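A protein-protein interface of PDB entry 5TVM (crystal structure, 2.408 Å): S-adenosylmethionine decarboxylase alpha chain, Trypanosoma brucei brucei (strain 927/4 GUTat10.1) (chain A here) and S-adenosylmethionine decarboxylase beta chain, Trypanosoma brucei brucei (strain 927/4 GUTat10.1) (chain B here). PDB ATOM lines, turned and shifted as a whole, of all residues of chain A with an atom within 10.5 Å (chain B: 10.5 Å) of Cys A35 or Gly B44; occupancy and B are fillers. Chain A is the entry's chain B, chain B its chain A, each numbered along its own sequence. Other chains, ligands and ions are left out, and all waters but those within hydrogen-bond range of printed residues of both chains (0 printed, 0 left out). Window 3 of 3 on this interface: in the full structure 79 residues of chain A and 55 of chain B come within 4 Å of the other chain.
The backbone NH of Met B39 sits at hydrogen-bond distance from the backbone carbonyl oxygen of Asp A8. The guanidinium group of Arg B40 is in salt-bridge range of the side-chain carboxylate of Glu A37, at 3.1 Å. The backbone carbonyl oxygen (O) of Cys A35 sits at hydrogen-bond distance from the side-chain hydroxyl (OG1) of Thr B45. The backbone NH (N) of His B46 sits at hydrogen-bond distance from the backbone carbonyl oxygen (O) of Val A34. The backbone NH of Leu B50 sits at hydrogen-bond distance from the backbone carbonyl oxygen of Lys A7 (3.0 Å). NE2 of His B53 lies within hydrogen-bond range of O of Ala A30 (2.7 Å).
N of Val B42 is in hydrogen-bond range of OG1 of Thr B45. ND1 of His B46 sits at hydrogen-bond distance from N of Ser B48 (3.0 Å). O of Glu A29 sits at hydrogen-bond distance from OG1 of Thr A33 (3.1 Å). The backbone carbonyl oxygen (O) of Val A31 is in hydrogen-bond range of the backbone NH (N) of Gly A36. The side-chain sulfur (SG) of Cys A35 lies within hydrogen-bond range of the backbone carbonyl oxygen (O) of Thr A33, at 3.8 Å.
Among the printed residues, merely in contact across the chains: Glu A37 with Met B39 (3.1 Å), Lys A7 with Gly B49 (3.3 Å), Val A34 with Gly B49 (3.3 Å), Cys A35 with Val B42 (3.4 Å), Val A34 with Thr B45 (3.4 Å), Val A34 with His B53 (3.4 Å), Ala A30 with Leu B50 (3.5 Å), Val A31 with Met B39 (3.5 Å), Cys A35 with Gly B44 (3.6 Å), Gly A36 with Arg B40 (3.6 Å), Lys A7 with Ser B48 (3.6 Å), Lys A7 with Met B39 (3.7 Å), Lys A7 with Leu B51 (3.7 Å), Thr A33 with His B53 (3.7 Å), Val A38 with Arg B40 (3.7 Å), Val A31 with Leu B50 (3.9 Å) and Val A34 with Met B39 (3.96 Å).
Gly B44 touches one residue of chain A. Thr A33 touches just one residue of chain B: His B53. Val B42 touches one residue of chain A. Of the printed residues of chain B, Lys A7 touches Met B39, Ser B48, Gly B49, Leu B50 and Leu B51. Of the printed residues of chain A, Leu B51 touches Lys A7 (3.7 Å). Val B47 touches none of the printed residues of chain A. Ile A27 touches none of the printed residues of chain B. The nearest residue of chain B that does not touch Cys A35 is His B46 (4.9 Å). The nearest residue of chain A that does not touch Gly B44 is Val A34 (4.3 Å).
Printed residues of chain A that touch a printed residue of chain B: Lys A7, Asp A8, Ala A30, Val A31, Thr A33, Val A34, Cys A35, Gly A36, Glu A37 and Val A38. Along chain A the printed residues that touch a printed residue of chain B span positions 7 to 38. Hydrophobic or aromatic side chains of chain B that line the printed part of chain A: Met B39, Val B42, His B46, Leu B50, Leu B51 and His B53. Among the printed residues, 23 pairs touch across the chains. Among the printed residues, Asp or Glu carboxylates within 4 Å of a Lys or Arg side-chain nitrogen of the other chain: Glu A37 with Arg B40 (3.1 Å).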
ATOM      1  N   LYS A   7      30.870 -28.992  19.021  1.00  0.00           N
ATOM      2  CA  LYS A   7      30.173 -28.598  20.238  1.00  0.00           C
ATOM      3  C   LYS A   7      30.736 -27.306  20.814  1.00  0.00           C
ATOM      4  O   LYS A   7      30.001 -26.538  21.446  1.00  0.00           O
ATOM      5  CB  LYS A   7      30.260 -29.716  21.276  1.00  0.00           C
ATOM      6  CG  LYS A   7      29.595 -29.385  22.607  1.00  0.00           C
ATOM      7  CD  LYS A   7      29.749 -30.514  23.617  1.00  0.00           C
ATOM      8  CE  LYS A   7      31.203 -30.711  24.028  1.00  0.00           C
ATOM      9  NZ  LYS A   7      31.354 -31.757  25.077  1.00  0.00           N
ATOM     10  N   ASP A   8      32.026 -27.041  20.603  1.00  0.00           N
ATOM     11  CA  ASP A   8      32.708 -25.964  21.303  1.00  0.00           C
ATOM     12  C   ASP A   8      33.431 -24.975  20.400  1.00  0.00           C
ATOM     13  O   ASP A   8      34.054 -24.043  20.921  1.00  0.00           O
ATOM     14  CB  ASP A   8      33.730 -26.544  22.291  1.00  0.00           C
ATOM     15  CG  ASP A   8      34.908 -27.192  21.588  1.00  0.00           C
ATOM     16  OD1 ASP A   8      34.767 -27.550  20.400  1.00  0.00           O
ATOM     17  OD2 ASP A   8      35.973 -27.342  22.222  1.00  0.00           O
ATOM     18  N   ILE A  27      29.428 -15.023  14.185  1.00  0.00           N
ATOM     19  CA  ILE A  27      29.961 -16.128  14.974  1.00  0.00           C
ATOM     20  C   ILE A  27      29.908 -15.793  16.458  1.00  0.00           C
ATOM     21  O   ILE A  27      29.572 -16.647  17.288  1.00  0.00           O
ATOM     22  CB  ILE A  27      31.389 -16.476  14.514  1.00  0.00           C
ATOM     23  CG1 ILE A  27      31.331 -17.189  13.156  1.00  0.00           C
ATOM     24  CG2 ILE A  27      32.102 -17.347  15.556  1.00  0.00           C
ATOM     25  CD1 ILE A  27      32.686 -17.523  12.556  1.00  0.00           C
ATOM     26  N   CYS A  28      30.251 -14.554  16.822  1.00  0.00           N
ATOM     27  CA  CYS A  28      30.101 -14.127  18.209  1.00  0.00           C
ATOM     28  C   CYS A  28      28.650 -14.234  18.655  1.00  0.00           C
ATOM     29  O   CYS A  28      28.368 -14.589  19.807  1.00  0.00           O
ATOM     30  CB  CYS A  28      30.604 -12.694  18.377  1.00  0.00           C
ATOM     31  SG  CYS A  28      32.372 -12.481  18.074  1.00  0.00           S
ATOM     32  N   GLU A  29      27.712 -13.930  17.755  1.00  0.00           N
ATOM     33  CA  GLU A  29      26.297 -14.042  18.089  1.00  0.00           C
ATOM     34  C   GLU A  29      25.887 -15.501  18.252  1.00  0.00           C
ATOM     35  O   GLU A  29      25.087 -15.831  19.135  1.00  0.00           O
ATOM     36  CB  GLU A  29      25.454 -13.365  17.009  1.00  0.00           C
ATOM     37  CG  GLU A  29      24.032 -13.047  17.440  1.00  0.00           C
ATOM     38  CD  GLU A  29      23.229 -12.370  16.345  1.00  0.00           C
ATOM     39  OE1 GLU A  29      23.377 -12.761  15.168  1.00  0.00           O
ATOM     40  OE2 GLU A  29      22.455 -11.442  16.662  1.00  0.00           O
ATOM     41  N   ALA A  30      26.424 -16.389  17.411  1.00  0.00           N
ATOM     42  CA  ALA A  30      26.104 -17.807  17.530  1.00  0.00           C
ATOM     43  C   ALA A  30      26.555 -18.368  18.871  1.00  0.00           C
ATOM     44  O   ALA A  30      25.940 -19.307  19.390  1.00  0.00           O
ATOM     45  CB  ALA A  30      26.746 -18.590  16.386  1.00  0.00           C
ATOM     46  N   VAL A  31      27.620 -17.808  19.446  1.00  0.00           N
ATOM     47  CA  VAL A  31      28.093 -18.267  20.747  1.00  0.00           C
ATOM     48  C   VAL A  31      27.246 -17.680  21.871  1.00  0.00           C
ATOM     49  O   VAL A  31      27.076 -18.316  22.918  1.00  0.00           O
ATOM     50  CB  VAL A  31      29.580 -17.911  20.918  1.00  0.00           C
ATOM     51  CG1 VAL A  31      30.063 -18.226  22.334  1.00  0.00           C
ATOM     52  CG2 VAL A  31      30.422 -18.657  19.894  1.00  0.00           C
ATOM     53  N   SER A  32      26.705 -16.473  21.684  1.00  0.00           N
ATOM     54  CA  SER A  32      25.917 -15.845  22.739  1.00  0.00           C
ATOM     55  C   SER A  32      24.558 -16.519  22.895  1.00  0.00           C
ATOM     56  O   SER A  32      24.073 -16.694  24.019  1.00  0.00           O
ATOM     57  CB  SER A  32      25.740 -14.355  22.446  1.00  0.00           C
ATOM     58  OG  SER A  32      24.915 -14.154  21.312  1.00  0.00           O
ATOM     59  N   THR A  33      23.930 -16.903  21.781  1.00  0.00           N
ATOM     60  CA  THR A  33      22.614 -17.533  21.845  1.00  0.00           C
ATOM     61  C   THR A  33      22.636 -18.765  22.742  1.00  0.00           C
ATOM     62  O   THR A  33      21.779 -18.924  23.620  1.00  0.00           O
ATOM     63  CB  THR A  33      22.143 -17.906  20.437  1.00  0.00           C
ATOM     64  OG1 THR A  33      22.136 -16.738  19.608  1.00  0.00           O
ATOM     65  CG2 THR A  33      20.740 -18.504  20.475  1.00  0.00           C
ATOM     66  N   VAL A  34      23.613 -19.646  22.538  1.00  0.00           N
ATOM     67  CA  VAL A  34      23.718 -20.883  23.306  1.00  0.00           C
ATOM     68  C   VAL A  34      24.325 -20.604  24.674  1.00  0.00           C
ATOM     69  O   VAL A  34      24.606 -21.536  25.439  1.00  0.00           O
ATOM     70  CB  VAL A  34      24.545 -21.939  22.550  1.00  0.00           C
ATOM     71  CG1 VAL A  34      23.880 -22.286  21.228  1.00  0.00           C
ATOM     72  CG2 VAL A  34      25.975 -21.450  22.324  1.00  0.00           C
ATOM     73  N   CYS A  35      24.545 -19.327  24.992  1.00  0.00           N
ATOM     74  CA  CYS A  35      25.073 -18.921  26.293  1.00  0.00           C
ATOM     75  C   CYS A  35      26.508 -19.410  26.486  1.00  0.00           C
ATOM     76  O   CYS A  35      26.872 -19.900  27.556  1.00  0.00           O
ATOM     77  CB  CYS A  35      24.173 -19.409  27.432  1.00  0.00           C
ATOM     78  SG  CYS A  35      22.479 -18.781  27.343  1.00  0.00           S
ATOM     79  N   GLY A  36      27.324 -19.279  25.439  1.00  0.00           N
ATOM     80  CA  GLY A  36      28.743 -19.530  25.530  1.00  0.00           C
ATOM     81  C   GLY A  36      29.529 -18.232  25.671  1.00  0.00           C
ATOM     82  O   GLY A  36      28.982 -17.133  25.702  1.00  0.00           O
ATOM     83  N   GLU A  37      30.849 -18.384  25.757  1.00  0.00           N
ATOM     84  CA  GLU A  37      31.747 -17.243  25.905  1.00  0.00           C
ATOM     85  C   GLU A  37      32.990 -17.482  25.068  1.00  0.00           C
ATOM     86  O   GLU A  37      33.710 -18.461  25.288  1.00  0.00           O
ATOM     87  CB  GLU A  37      32.123 -17.024  27.373  1.00  0.00           C
ATOM     88  CG  GLU A  37      30.963 -16.571  28.243  1.00  0.00           C
ATOM     89  CD  GLU A  37      31.365 -16.354  29.687  1.00  0.00           C
ATOM     90  OE1 GLU A  37      32.470 -16.793  30.072  1.00  0.00           O
ATOM     91  OE2 GLU A  37      30.576 -15.741  30.438  1.00  0.00           O
ATOM     92  N   VAL A  38      33.242 -16.587  24.109  1.00  0.00           N
ATOM     93  CA  VAL A  38      34.456 -16.682  23.309  1.00  0.00           C
ATOM     94  C   VAL A  38      35.664 -16.607  24.229  1.00  0.00           C
ATOM     95  O   VAL A  38      35.734 -15.752  25.121  1.00  0.00           O
ATOM     96  CB  VAL A  38      34.489 -15.569  22.250  1.00  0.00           C
ATOM     97  CG1 VAL A  38      35.789 -15.629  21.448  1.00  0.00           C
ATOM     98  CG2 VAL A  38      33.284 -15.677  21.324  1.00  0.00           C
ATOM     99  N   MET B  39      34.746 -21.494  22.223  1.00  0.00           N
ATOM    100  CA  MET B  39      33.951 -20.838  23.250  1.00  0.00           C
ATOM    101  C   MET B  39      34.084 -21.566  24.583  1.00  0.00           C
ATOM    102  O   MET B  39      34.358 -22.769  24.633  1.00  0.00           O
ATOM    103  CB  MET B  39      32.471 -20.773  22.847  1.00  0.00           C
ATOM    104  CG  MET B  39      31.717 -22.096  22.946  1.00  0.00           C
ATOM    105  SD  MET B  39      29.971 -21.909  22.536  1.00  0.00           S
ATOM    106  CE  MET B  39      29.294 -23.423  23.214  1.00  0.00           C
ATOM    107  N   ARG B  40      33.884 -20.814  25.662  1.00  0.00           N
ATOM    108  CA  ARG B  40      33.830 -21.375  27.001  1.00  0.00           C
ATOM    109  C   ARG B  40      32.435 -21.929  27.279  1.00  0.00           C
ATOM    110  O   ARG B  40      31.461 -21.602  26.597  1.00  0.00           O
ATOM    111  CB  ARG B  40      34.185 -20.311  28.040  1.00  0.00           C
ATOM    112  CG  ARG B  40      35.186 -20.762  29.093  1.00  0.00           C
ATOM    113  CD  ARG B  40      35.310 -19.735  30.212  1.00  0.00           C
ATOM    114  NE  ARG B  40      35.135 -18.370  29.724  1.00  0.00           N
ATOM    115  CZ  ARG B  40      36.106 -17.620  29.209  1.00  0.00           C
ATOM    116  NH1 ARG B  40      37.342 -18.095  29.108  1.00  0.00           N
ATOM    117  NH2 ARG B  40      35.841 -16.390  28.792  1.00  0.00           N
ATOM    118  N   VAL B  41      32.348 -22.774  28.303  1.00  0.00           N
ATOM    119  CA  VAL B  41      31.092 -23.399  28.707  1.00  0.00           C
ATOM    120  C   VAL B  41      30.793 -22.951  30.131  1.00  0.00           C
ATOM    121  O   VAL B  41      31.487 -23.353  31.075  1.00  0.00           O
ATOM    122  CB  VAL B  41      31.155 -24.930  28.610  1.00  0.00           C
ATOM    123  CG1 VAL B  41      29.874 -25.561  29.149  1.00  0.00           C
ATOM    124  CG2 VAL B  41      31.390 -25.359  27.169  1.00  0.00           C
ATOM    125  N   VAL B  42      29.761 -22.123  30.288  1.00  0.00           N
ATOM    126  CA  VAL B  42      29.294 -21.708  31.606  1.00  0.00           C
ATOM    127  C   VAL B  42      28.197 -22.675  32.033  1.00  0.00           C
ATOM    128  O   VAL B  42      27.729 -23.488  31.228  1.00  0.00           O
ATOM    129  CB  VAL B  42      28.803 -20.244  31.592  1.00  0.00           C
ATOM    130  CG1 VAL B  42      27.467 -20.115  30.864  1.00  0.00           C
ATOM    131  CG2 VAL B  42      28.721 -19.670  33.008  1.00  0.00           C
ATOM    132  N   ASP B  43      27.794 -22.609  33.304  1.00  0.00           N
ATOM    133  CA  ASP B  43      26.726 -23.473  33.800  1.00  0.00           C
ATOM    134  C   ASP B  43      25.506 -23.433  32.885  1.00  0.00           C
ATOM    135  O   ASP B  43      24.929 -24.474  32.550  1.00  0.00           O
ATOM    136  CB  ASP B  43      26.341 -23.058  35.222  1.00  0.00           C
ATOM    137  CG  ASP B  43      27.508 -23.133  36.187  1.00  0.00           C
ATOM    138  OD1 ASP B  43      28.303 -24.090  36.089  1.00  0.00           O
ATOM    139  OD2 ASP B  43      27.632 -22.232  37.044  1.00  0.00           O
ATOM    140  N   GLY B  44      25.100 -22.236  32.470  1.00  0.00           N
ATOM    141  CA  GLY B  44      23.920 -22.066  31.648  1.00  0.00           C
ATOM    142  C   GLY B  44      24.089 -22.357  30.175  1.00  0.00           C
ATOM    143  O   GLY B  44      23.134 -22.187  29.412  1.00  0.00           O
ATOM    144  N   THR B  45      25.270 -22.789  29.742  1.00  0.00           N
ATOM    145  CA  THR B  45      25.489 -23.069  28.329  1.00  0.00           C
ATOM    146  C   THR B  45      24.662 -24.269  27.890  1.00  0.00           C
ATOM    147  O   THR B  45      24.491 -25.237  28.637  1.00  0.00           O
ATOM    148  CB  THR B  45      26.971 -23.333  28.057  1.00  0.00           C
ATOM    149  OG1 THR B  45      27.735 -22.168  28.386  1.00  0.00           O
ATOM    150  CG2 THR B  45      27.203 -23.685  26.588  1.00  0.00           C
ATOM    151  N   HIS B  46      24.149 -24.199  26.664  1.00  0.00           N
ATOM    152  CA  HIS B  46      23.410 -25.315  26.092  1.00  0.00           C
ATOM    153  C   HIS B  46      24.261 -26.578  26.128  1.00  0.00           C
ATOM    154  O   HIS B  46      25.451 -26.555  25.796  1.00  0.00           O
ATOM    155  CB  HIS B  46      23.002 -24.990  24.653  1.00  0.00           C
ATOM    156  CG  HIS B  46      21.839 -25.791  24.157  1.00  0.00           C
ATOM    157  ND1 HIS B  46      21.945 -27.118  23.802  1.00  0.00           N
ATOM    158  CD2 HIS B  46      20.546 -25.449  23.948  1.00  0.00           C
ATOM    159  CE1 HIS B  46      20.768 -27.561  23.402  1.00  0.00           C
ATOM    160  NE2 HIS B  46      19.900 -26.569  23.480  1.00  0.00           N
ATOM    161  N   VAL B  47      23.646 -27.689  26.543  1.00  0.00           N
ATOM    162  CA  VAL B  47      24.378 -28.946  26.673  1.00  0.00           C
ATOM    163  C   VAL B  47      24.926 -29.413  25.333  1.00  0.00           C
ATOM    164  O   VAL B  47      25.900 -30.172  25.292  1.00  0.00           O
ATOM    165  CB  VAL B  47      23.470 -30.024  27.304  1.00  0.00           C
ATOM    166  CG1 VAL B  47      24.230 -31.334  27.482  1.00  0.00           C
ATOM    167  CG2 VAL B  47      22.919 -29.540  28.643  1.00  0.00           C
ATOM    168  N   SER B  48      24.320 -28.979  24.229  1.00  0.00           N
ATOM    169  CA  SER B  48      24.791 -29.314  22.892  1.00  0.00           C
ATOM    170  C   SER B  48      25.794 -28.308  22.348  1.00  0.00           C
ATOM    171  O   SER B  48      26.372 -28.550  21.283  1.00  0.00           O
ATOM    172  CB  SER B  48      23.604 -29.413  21.925  1.00  0.00           C
ATOM    173  OG  SER B  48      22.662 -30.373  22.366  1.00  0.00           O
ATOM    174  N   GLY B  49      26.011 -27.193  23.042  1.00  0.00           N
ATOM    175  CA  GLY B  49      26.964 -26.204  22.566  1.00  0.00           C
ATOM    176  C   GLY B  49      26.498 -25.568  21.271  1.00  0.00           C
ATOM    177  O   GLY B  49      25.310 -25.291  21.074  1.00  0.00           O
ATOM    178  N   LEU B  50      27.450 -25.332  20.367  1.00  0.00           N
ATOM    179  CA  LEU B  50      27.126 -24.723  19.083  1.00  0.00           C
ATOM    180  C   LEU B  50      26.351 -25.666  18.173  1.00  0.00           C
ATOM    181  O   LEU B  50      25.718 -25.201  17.219  1.00  0.00           O
ATOM    182  CB  LEU B  50      28.407 -24.260  18.386  1.00  0.00           C
ATOM    183  CG  LEU B  50      29.110 -23.063  19.030  1.00  0.00           C
ATOM    184  CD1 LEU B  50      30.540 -22.935  18.531  1.00  0.00           C
ATOM    185  CD2 LEU B  50      28.340 -21.782  18.753  1.00  0.00           C
ATOM    186  N   LEU B  51      26.384 -26.974  18.442  1.00  0.00           N
ATOM    187  CA  LEU B  51      25.616 -27.929  17.654  1.00  0.00           C
ATOM    188  C   LEU B  51      24.113 -27.783  17.856  1.00  0.00           C
ATOM    189  O   LEU B  51      23.344 -28.363  17.082  1.00  0.00           O
ATOM    190  CB  LEU B  51      26.044 -29.356  18.000  1.00  0.00           C
ATOM    191  CG  LEU B  51      27.495 -29.717  17.670  1.00  0.00           C
ATOM    192  CD1 LEU B  51      27.888 -31.025  18.335  1.00  0.00           C
ATOM    193  CD2 LEU B  51      27.696 -29.808  16.166  1.00  0.00           C
ATOM    194  N   ALA B  52      23.679 -27.034  18.872  1.00  0.00           N
ATOM    195  CA  ALA B  52      22.252 -26.803  19.064  1.00  0.00           C
ATOM    196  C   ALA B  52      21.656 -26.008  17.910  1.00  0.00           C
ATOM    197  O   ALA B  52      20.460 -26.132  17.622  1.00  0.00           O
ATOM    198  CB  ALA B  52      22.013 -26.073  20.385  1.00  0.00           C
ATOM    199  N   HIS B  53      22.465 -25.191  17.242  1.00  0.00           N
ATOM    200  CA  HIS B  53      21.977 -24.406  16.118  1.00  0.00           C
ATOM    201  C   HIS B  53      21.615 -25.311  14.947  1.00  0.00           C
ATOM    202  O   HIS B  53      22.279 -26.320  14.692  1.00  0.00           O
ATOM    203  CB  HIS B  53      23.034 -23.394  15.675  1.00  0.00           C
ATOM    204  CG  HIS B  53      23.295 -22.311  16.674  1.00  0.00           C
ATOM    205  ND1 HIS B  53      22.338 -21.387  17.037  1.00  0.00           N
ATOM    206  CD2 HIS B  53      24.409 -21.992  17.374  1.00  0.00           C
ATOM    207  CE1 HIS B  53      22.850 -20.552  17.923  1.00  0.00           C
ATOM    208  NE2 HIS B  53      24.105 -20.896  18.145  1.00  0.00           N
